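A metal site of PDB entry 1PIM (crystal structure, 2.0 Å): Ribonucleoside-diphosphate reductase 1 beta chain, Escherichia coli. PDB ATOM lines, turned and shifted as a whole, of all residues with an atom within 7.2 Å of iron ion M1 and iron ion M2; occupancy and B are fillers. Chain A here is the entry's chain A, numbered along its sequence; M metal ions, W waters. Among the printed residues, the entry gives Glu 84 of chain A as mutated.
Trp 111 touches iron ion M2 (NE1 to FE, 3.9 Å).
Of the 23 residues printed, 5 come within 4 Å of iron ion M2.
The nearest printed residue that does not touch iron ion M2 is Gln 87 (4.8 Å).
Iron ion M1 is bound by OE1 of Glu 115 (2.1 Å), OE1 of Glu 84 (2.2 Å), ND1 of His 118 (2.3 Å), OE2 of Glu 238 (2.5 Å) and OE2 of Glu 84 (2.5 Å).
The side-chain carboxylate (OE2) of Glu 204 is bound to iron ion M2 (2.2 Å).
Water W1 binds iron ion M2, at 2.2 Å.
The side-chain carboxylate (OE2) of Glu 115 binds iron ion M2, at 2.2 Å.
Iron ion M2 is bound by ND1 of His 241 (2.3 Å).
OE2 of Glu 238 binds iron ion M2, 2.3 Å away.
OE1 of Glu 238 is bound to iron ion M2 (2.4 Å).
Of the 23 residues printed, 4 come within 4 Å of iron ion M1.
The nearest printed residue that does not touch iron ion M1 is Phe 208 (4.4 Å).
The indole nitrogen (NE1) of Trp 111 lies close to the side-chain carboxylate (OE2) of Glu 115, 3.2 Å away.
The backbone carbonyl oxygen (O) of Glu 115 is in hydrogen-bond range of the side-chain hydroxyl (OG) of Ser 119, at 3.4 Å.
The side-chain hydroxyl of Ser 114 is in hydrogen-bond range of the backbone carbonyl oxygen of Trp 111 (2.6 Å).
OE2 of Glu 204 sits close to NE2 of Gln 87, 3.2 Å away.
NE2 of His 241 lies within hydrogen-bond range of OG of Ser 114 (2.9 Å).
A ring nitrogen (NE2) of His 118 lies within hydrogen-bond range of the side-chain carboxylate (OD2) of Asp 237 (2.9 Å).
OG of Ser 119 lies close to O of Glu 84.
The indole nitrogen (NE1) of Trp 111 sits close to the side-chain carboxylate (OE2) of Glu 204 (3.0 Å).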
ATOM      1  N   GLN A  80      24.007   4.459 -15.003  1.00  0.00           N
ATOM      2  CA  GLN A  80      23.788   5.059 -13.701  1.00  0.00           C
ATOM      3  C   GLN A  80      24.670   6.309 -13.583  1.00  0.00           C
ATOM      4  O   GLN A  80      24.235   7.356 -13.083  1.00  0.00           O
ATOM      5  CB  GLN A  80      24.133   4.075 -12.575  1.00  0.00           C
ATOM      6  CG  GLN A  80      23.220   2.837 -12.497  1.00  0.00           C
ATOM      7  CD  GLN A  80      23.690   1.792 -11.487  1.00  0.00           C
ATOM      8  OE1 GLN A  80      24.848   1.384 -11.497  1.00  0.00           O
ATOM      9  NE2 GLN A  80      22.774   1.328 -10.634  1.00  0.00           N
ATOM     10  N   LEU A  83      23.280   9.290 -15.603  1.00  0.00           N
ATOM     11  CA  LEU A  83      22.102   9.874 -14.971  1.00  0.00           C
ATOM     12  C   LEU A  83      22.466  10.734 -13.756  1.00  0.00           C
ATOM     13  O   LEU A  83      21.873  11.788 -13.523  1.00  0.00           O
ATOM     14  CB  LEU A  83      21.116   8.783 -14.567  1.00  0.00           C
ATOM     15  CG  LEU A  83      20.568   7.861 -15.666  1.00  0.00           C
ATOM     16  CD1 LEU A  83      19.530   6.921 -15.065  1.00  0.00           C
ATOM     17  CD2 LEU A  83      19.949   8.674 -16.790  1.00  0.00           C
ATOM     18  N   GLU A  84      23.452  10.284 -12.974  1.00  0.00           N
ATOM     19  CA  GLU A  84      23.863  11.026 -11.790  1.00  0.00           C
ATOM     20  C   GLU A  84      24.648  12.271 -12.184  1.00  0.00           C
ATOM     21  O   GLU A  84      24.608  13.280 -11.474  1.00  0.00           O
ATOM     22  CB  GLU A  84      24.699  10.134 -10.864  1.00  0.00           C
ATOM     23  CG  GLU A  84      23.973   8.863 -10.443  1.00  0.00           C
ATOM     24  CD  GLU A  84      23.045   9.057  -9.251  1.00  0.00           C
ATOM     25  OE1 GLU A  84      22.510  10.170  -9.064  1.00  0.00           O
ATOM     26  OE2 GLU A  84      22.835   8.072  -8.507  1.00  0.00           O
ATOM     27  N   GLN A  87      21.961  14.654 -12.870  1.00  0.00           N
ATOM     28  CA  GLN A  87      21.235  14.979 -11.634  1.00  0.00           C
ATOM     29  C   GLN A  87      22.047  15.780 -10.627  1.00  0.00           C
ATOM     30  O   GLN A  87      21.506  16.452  -9.765  1.00  0.00           O
ATOM     31  CB  GLN A  87      20.712  13.703 -10.964  1.00  0.00           C
ATOM     32  CG  GLN A  87      19.472  13.101 -11.617  1.00  0.00           C
ATOM     33  CD  GLN A  87      18.289  14.075 -11.639  1.00  0.00           C
ATOM     34  OE1 GLN A  87      18.100  14.831 -12.592  1.00  0.00           O
ATOM     35  NE2 GLN A  87      17.506  14.070 -10.564  1.00  0.00           N
ATOM     36  N   TRP A 111      19.348  17.871  -2.138  1.00  0.00           N
ATOM     37  CA  TRP A 111      19.072  16.781  -3.071  1.00  0.00           C
ATOM     38  C   TRP A 111      20.186  16.699  -4.115  1.00  0.00           C
ATOM     39  O   TRP A 111      20.737  15.628  -4.357  1.00  0.00           O
ATOM     40  CB  TRP A 111      17.693  17.046  -3.693  1.00  0.00           C
ATOM     41  CG  TRP A 111      17.320  16.323  -4.936  1.00  0.00           C
ATOM     42  CD1 TRP A 111      17.794  15.117  -5.369  1.00  0.00           C
ATOM     43  CD2 TRP A 111      16.300  16.708  -5.864  1.00  0.00           C
ATOM     44  NE1 TRP A 111      17.124  14.729  -6.520  1.00  0.00           N
ATOM     45  CE2 TRP A 111      16.211  15.688  -6.838  1.00  0.00           C
ATOM     46  CE3 TRP A 111      15.454  17.829  -5.968  1.00  0.00           C
ATOM     47  CZ2 TRP A 111      15.295  15.754  -7.904  1.00  0.00           C
ATOM     48  CZ3 TRP A 111      14.545  17.882  -7.031  1.00  0.00           C
ATOM     49  CH2 TRP A 111      14.481  16.849  -7.985  1.00  0.00           C
ATOM     50  N   SER A 114      23.436  15.442  -2.632  1.00  0.00           N
ATOM     51  CA  SER A 114      23.444  13.993  -2.466  1.00  0.00           C
ATOM     52  C   SER A 114      23.744  13.297  -3.787  1.00  0.00           C
ATOM     53  O   SER A 114      24.366  12.234  -3.804  1.00  0.00           O
ATOM     54  CB  SER A 114      22.104  13.487  -1.874  1.00  0.00           C
ATOM     55  OG  SER A 114      21.044  13.586  -2.797  1.00  0.00           O
ATOM     56  N   GLU A 115      23.353  13.897  -4.916  1.00  0.00           N
ATOM     57  CA  GLU A 115      23.629  13.303  -6.217  1.00  0.00           C
ATOM     58  C   GLU A 115      25.136  13.304  -6.504  1.00  0.00           C
ATOM     59  O   GLU A 115      25.644  12.342  -7.090  1.00  0.00           O
ATOM     60  CB  GLU A 115      22.879  14.039  -7.338  1.00  0.00           C
ATOM     61  CG  GLU A 115      21.374  14.108  -7.150  1.00  0.00           C
ATOM     62  CD  GLU A 115      20.697  12.744  -7.215  1.00  0.00           C
ATOM     63  OE1 GLU A 115      21.389  11.729  -7.040  1.00  0.00           O
ATOM     64  OE2 GLU A 115      19.473  12.690  -7.446  1.00  0.00           O
ATOM     65  N   THR A 116      25.855  14.349  -6.095  1.00  0.00           N
ATOM     66  CA  THR A 116      27.282  14.377  -6.371  1.00  0.00           C
ATOM     67  C   THR A 116      27.983  13.297  -5.545  1.00  0.00           C
ATOM     68  O   THR A 116      29.060  12.820  -5.905  1.00  0.00           O
ATOM     69  CB  THR A 116      27.953  15.773  -6.087  1.00  0.00           C
ATOM     70  OG1 THR A 116      27.978  16.038  -4.681  1.00  0.00           O
ATOM     71  CG2 THR A 116      27.187  16.882  -6.817  1.00  0.00           C
ATOM     72  N   ILE A 117      27.368  12.904  -4.426  1.00  0.00           N
ATOM     73  CA  ILE A 117      27.926  11.847  -3.603  1.00  0.00           C
ATOM     74  C   ILE A 117      27.749  10.522  -4.365  1.00  0.00           C
ATOM     75  O   ILE A 117      28.644   9.676  -4.370  1.00  0.00           O
ATOM     76  CB  ILE A 117      27.223  11.760  -2.233  1.00  0.00           C
ATOM     77  CG1 ILE A 117      27.513  13.028  -1.422  1.00  0.00           C
ATOM     78  CG2 ILE A 117      27.663  10.490  -1.488  1.00  0.00           C
ATOM     79  CD1 ILE A 117      29.011  13.276  -1.144  1.00  0.00           C
ATOM     80  N   HIS A 118      26.589  10.360  -4.998  1.00  0.00           N
ATOM     81  CA  HIS A 118      26.329   9.146  -5.768  1.00  0.00           C
ATOM     82  C   HIS A 118      27.324   9.058  -6.920  1.00  0.00           C
ATOM     83  O   HIS A 118      27.929   7.997  -7.144  1.00  0.00           O
ATOM     84  CB  HIS A 118      24.877   9.135  -6.273  1.00  0.00           C
ATOM     85  CG  HIS A 118      23.861   9.095  -5.173  1.00  0.00           C
ATOM     86  ND1 HIS A 118      22.510   9.232  -5.402  1.00  0.00           N
ATOM     87  CD2 HIS A 118      24.001   8.916  -3.839  1.00  0.00           C
ATOM     88  CE1 HIS A 118      21.864   9.149  -4.251  1.00  0.00           C
ATOM     89  NE2 HIS A 118      22.752   8.962  -3.287  1.00  0.00           N
ATOM     90  N   SER A 119      27.524  10.169  -7.646  1.00  0.00           N
ATOM     91  CA  SER A 119      28.477  10.197  -8.754  1.00  0.00           C
ATOM     92  C   SER A 119      29.845   9.783  -8.243  1.00  0.00           C
ATOM     93  O   SER A 119      30.559   9.018  -8.901  1.00  0.00           O
ATOM     94  CB  SER A 119      28.563  11.597  -9.372  1.00  0.00           C
ATOM     95  OG  SER A 119      27.348  11.978  -9.983  1.00  0.00           O
ATOM     96  N   TYR A 122      30.285   6.072  -7.748  1.00  0.00           N
ATOM     97  CA  TYR A 122      30.539   5.299  -8.969  1.00  0.00           C
ATOM     98  C   TYR A 122      32.013   5.345  -9.397  1.00  0.00           C
ATOM     99  O   TYR A 122      32.507   4.384  -9.986  1.00  0.00           O
ATOM    100  CB  TYR A 122      29.647   5.786 -10.110  1.00  0.00           C
ATOM    101  CG  TYR A 122      28.174   5.513  -9.874  1.00  0.00           C
ATOM    102  CD1 TYR A 122      27.730   4.240  -9.516  1.00  0.00           C
ATOM    103  CD2 TYR A 122      27.228   6.529  -9.982  1.00  0.00           C
ATOM    104  CE1 TYR A 122      26.391   3.984  -9.269  1.00  0.00           C
ATOM    105  CE2 TYR A 122      25.874   6.290  -9.736  1.00  0.00           C
ATOM    106  CZ  TYR A 122      25.467   5.018  -9.384  1.00  0.00           C
ATOM    107  OH  TYR A 122      24.128   4.780  -9.135  1.00  0.00           O
ATOM    108  N   LEU A 203      12.592   9.691 -13.983  1.00  0.00           N
ATOM    109  CA  LEU A 203      14.004   9.325 -13.925  1.00  0.00           C
ATOM    110  C   LEU A 203      14.380   8.622 -12.619  1.00  0.00           C
ATOM    111  O   LEU A 203      15.009   7.565 -12.630  1.00  0.00           O
ATOM    112  CB  LEU A 203      14.874  10.566 -14.131  1.00  0.00           C
ATOM    113  CG  LEU A 203      16.400  10.425 -14.053  1.00  0.00           C
ATOM    114  CD1 LEU A 203      16.884   9.296 -14.946  1.00  0.00           C
ATOM    115  CD2 LEU A 203      17.053  11.735 -14.465  1.00  0.00           C
ATOM    116  N   GLU A 204      13.989   9.200 -11.489  1.00  0.00           N
ATOM    117  CA  GLU A 204      14.344   8.619 -10.185  1.00  0.00           C
ATOM    118  C   GLU A 204      13.426   7.516  -9.670  1.00  0.00           C
ATOM    119  O   GLU A 204      13.857   6.660  -8.890  1.00  0.00           O
ATOM    120  CB  GLU A 204      14.439   9.736  -9.149  1.00  0.00           C
ATOM    121  CG  GLU A 204      15.483  10.788  -9.511  1.00  0.00           C
ATOM    122  CD  GLU A 204      15.585  11.900  -8.479  1.00  0.00           C
ATOM    123  OE1 GLU A 204      14.533  12.456  -8.097  1.00  0.00           O
ATOM    124  OE2 GLU A 204      16.719  12.217  -8.077  1.00  0.00           O
ATOM    125  N   PHE A 208      15.997   4.596 -12.374  1.00  0.00           N
ATOM    126  CA  PHE A 208      16.964   4.168 -11.384  1.00  0.00           C
ATOM    127  C   PHE A 208      16.634   2.847 -10.708  1.00  0.00           C
ATOM    128  O   PHE A 208      17.521   2.062 -10.399  1.00  0.00           O
ATOM    129  CB  PHE A 208      17.186   5.256 -10.339  1.00  0.00           C
ATOM    130  CG  PHE A 208      18.397   6.088 -10.600  1.00  0.00           C
ATOM    131  CD1 PHE A 208      19.671   5.510 -10.583  1.00  0.00           C
ATOM    132  CD2 PHE A 208      18.284   7.433 -10.921  1.00  0.00           C
ATOM    133  CE1 PHE A 208      20.802   6.253 -10.884  1.00  0.00           C
ATOM    134  CE2 PHE A 208      19.410   8.195 -11.234  1.00  0.00           C
ATOM    135  CZ  PHE A 208      20.674   7.598 -11.207  1.00  0.00           C
ATOM    136  N   PHE A 212      18.810  -0.796 -10.222  1.00  0.00           N
ATOM    137  CA  PHE A 212      19.053  -1.434  -8.934  1.00  0.00           C
ATOM    138  C   PHE A 212      18.819  -2.941  -9.039  1.00  0.00           C
ATOM    139  O   PHE A 212      19.534  -3.728  -8.421  1.00  0.00           O
ATOM    140  CB  PHE A 212      18.103  -0.878  -7.852  1.00  0.00           C
ATOM    141  CG  PHE A 212      18.250   0.594  -7.602  1.00  0.00           C
ATOM    142  CD1 PHE A 212      19.476   1.232  -7.793  1.00  0.00           C
ATOM    143  CD2 PHE A 212      17.173   1.344  -7.143  1.00  0.00           C
ATOM    144  CE1 PHE A 212      19.625   2.596  -7.518  1.00  0.00           C
ATOM    145  CE2 PHE A 212      17.306   2.702  -6.863  1.00  0.00           C
ATOM    146  CZ  PHE A 212      18.539   3.328  -7.050  1.00  0.00           C
ATOM    147  N   ILE A 234      22.420   4.196  -1.894  1.00  0.00           N
ATOM    148  CA  ILE A 234      21.908   5.097  -2.920  1.00  0.00           C
ATOM    149  C   ILE A 234      20.376   4.957  -2.982  1.00  0.00           C
ATOM    150  O   ILE A 234      19.652   5.953  -3.002  1.00  0.00           O
ATOM    151  CB  ILE A 234      22.538   4.772  -4.310  1.00  0.00           C
ATOM    152  CG1 ILE A 234      24.023   5.162  -4.300  1.00  0.00           C
ATOM    153  CG2 ILE A 234      21.795   5.514  -5.425  1.00  0.00           C
ATOM    154  CD1 ILE A 234      24.763   4.790  -5.577  1.00  0.00           C
ATOM    155  N   ASP A 237      18.514   6.814  -0.474  1.00  0.00           N
ATOM    156  CA  ASP A 237      18.393   8.245  -0.743  1.00  0.00           C
ATOM    157  C   ASP A 237      17.345   8.485  -1.823  1.00  0.00           C
ATOM    158  O   ASP A 237      16.494   9.363  -1.686  1.00  0.00           O
ATOM    159  CB  ASP A 237      19.717   8.843  -1.227  1.00  0.00           C
ATOM    160  CG  ASP A 237      20.806   8.809  -0.170  1.00  0.00           C
ATOM    161  OD1 ASP A 237      20.517   9.051   1.011  1.00  0.00           O
ATOM    162  OD2 ASP A 237      21.975   8.568  -0.546  1.00  0.00           O
ATOM    163  N   GLU A 238      17.418   7.695  -2.901  1.00  0.00           N
ATOM    164  CA  GLU A 238      16.491   7.836  -4.022  1.00  0.00           C
ATOM    165  C   GLU A 238      15.014   7.822  -3.619  1.00  0.00           C
ATOM    166  O   GLU A 238      14.201   8.483  -4.260  1.00  0.00           O
ATOM    167  CB  GLU A 238      16.734   6.740  -5.063  1.00  0.00           C
ATOM    168  CG  GLU A 238      18.004   6.961  -5.858  1.00  0.00           C
ATOM    169  CD  GLU A 238      18.100   8.381  -6.402  1.00  0.00           C
ATOM    170  OE1 GLU A 238      17.130   8.817  -7.070  1.00  0.00           O
ATOM    171  OE2 GLU A 238      19.126   9.058  -6.154  1.00  0.00           O
ATOM    172  N   ALA A 239      14.694   7.073  -2.569  1.00  0.00           N
ATOM    173  CA  ALA A 239      13.317   6.998  -2.082  1.00  0.00           C
ATOM    174  C   ALA A 239      12.907   8.372  -1.540  1.00  0.00           C
ATOM    175  O   ALA A 239      11.729   8.762  -1.631  1.00  0.00           O
ATOM    176  CB  ALA A 239      13.221   5.937  -0.979  1.00  0.00           C
ATOM    177  N   LEU A 240      13.867   9.092  -0.964  1.00  0.00           N
ATOM    178  CA  LEU A 240      13.584  10.431  -0.459  1.00  0.00           C
ATOM    179  C   LEU A 240      13.383  11.393  -1.634  1.00  0.00           C
ATOM    180  O   LEU A 240      12.472  12.226  -1.617  1.00  0.00           O
ATOM    181  CB  LEU A 240      14.754  10.962   0.403  1.00  0.00           C
ATOM    182  CG  LEU A 240      15.081  10.294   1.747  1.00  0.00           C
ATOM    183  CD1 LEU A 240      16.195  11.083   2.440  1.00  0.00           C
ATOM    184  CD2 LEU A 240      13.842  10.284   2.631  1.00  0.00           C
ATOM    185  N   HIS A 241      14.239  11.286  -2.636  1.00  0.00           N
ATOM    186  CA  HIS A 241      14.150  12.162  -3.804  1.00  0.00           C
ATOM    187  C   HIS A 241      12.830  12.011  -4.550  1.00  0.00           C
ATOM    188  O   HIS A 241      12.202  13.012  -4.903  1.00  0.00           O
ATOM    189  CB  HIS A 241      15.301  11.880  -4.779  1.00  0.00           C
ATOM    190  CG  HIS A 241      16.663  11.987  -4.161  1.00  0.00           C
ATOM    191  ND1 HIS A 241      17.823  11.653  -4.840  1.00  0.00           N
ATOM    192  CD2 HIS A 241      17.054  12.362  -2.919  1.00  0.00           C
ATOM    193  CE1 HIS A 241      18.856  11.824  -4.043  1.00  0.00           C
ATOM    194  NE2 HIS A 241      18.427  12.246  -2.872  1.00  0.00           N
ATOM    195  N   LEU A 242      12.402  10.772  -4.772  1.00  0.00           N
ATOM    196  CA  LEU A 242      11.163  10.556  -5.495  1.00  0.00           C
ATOM    197  C   LEU A 242       9.967  11.024  -4.672  1.00  0.00           C
ATOM    198  O   LEU A 242       8.944  11.406  -5.235  1.00  0.00           O
ATOM    199  CB  LEU A 242      11.010   9.077  -5.888  1.00  0.00           C
ATOM    200  CG  LEU A 242      10.706   8.025  -4.826  1.00  0.00           C
ATOM    201  CD1 LEU A 242       9.205   8.012  -4.535  1.00  0.00           C
ATOM    202  CD2 LEU A 242      11.147   6.653  -5.335  1.00  0.00           C
HETATM  203 FE    FE M   1      21.263   9.605  -7.281  1.00  0.00          FE
HETATM  204 FE    FE M   2      18.118  10.966  -6.973  1.00  0.00          FE
HETATM  205  O   HOH W   1      18.836  10.146  -8.895  1.00  0.00           O
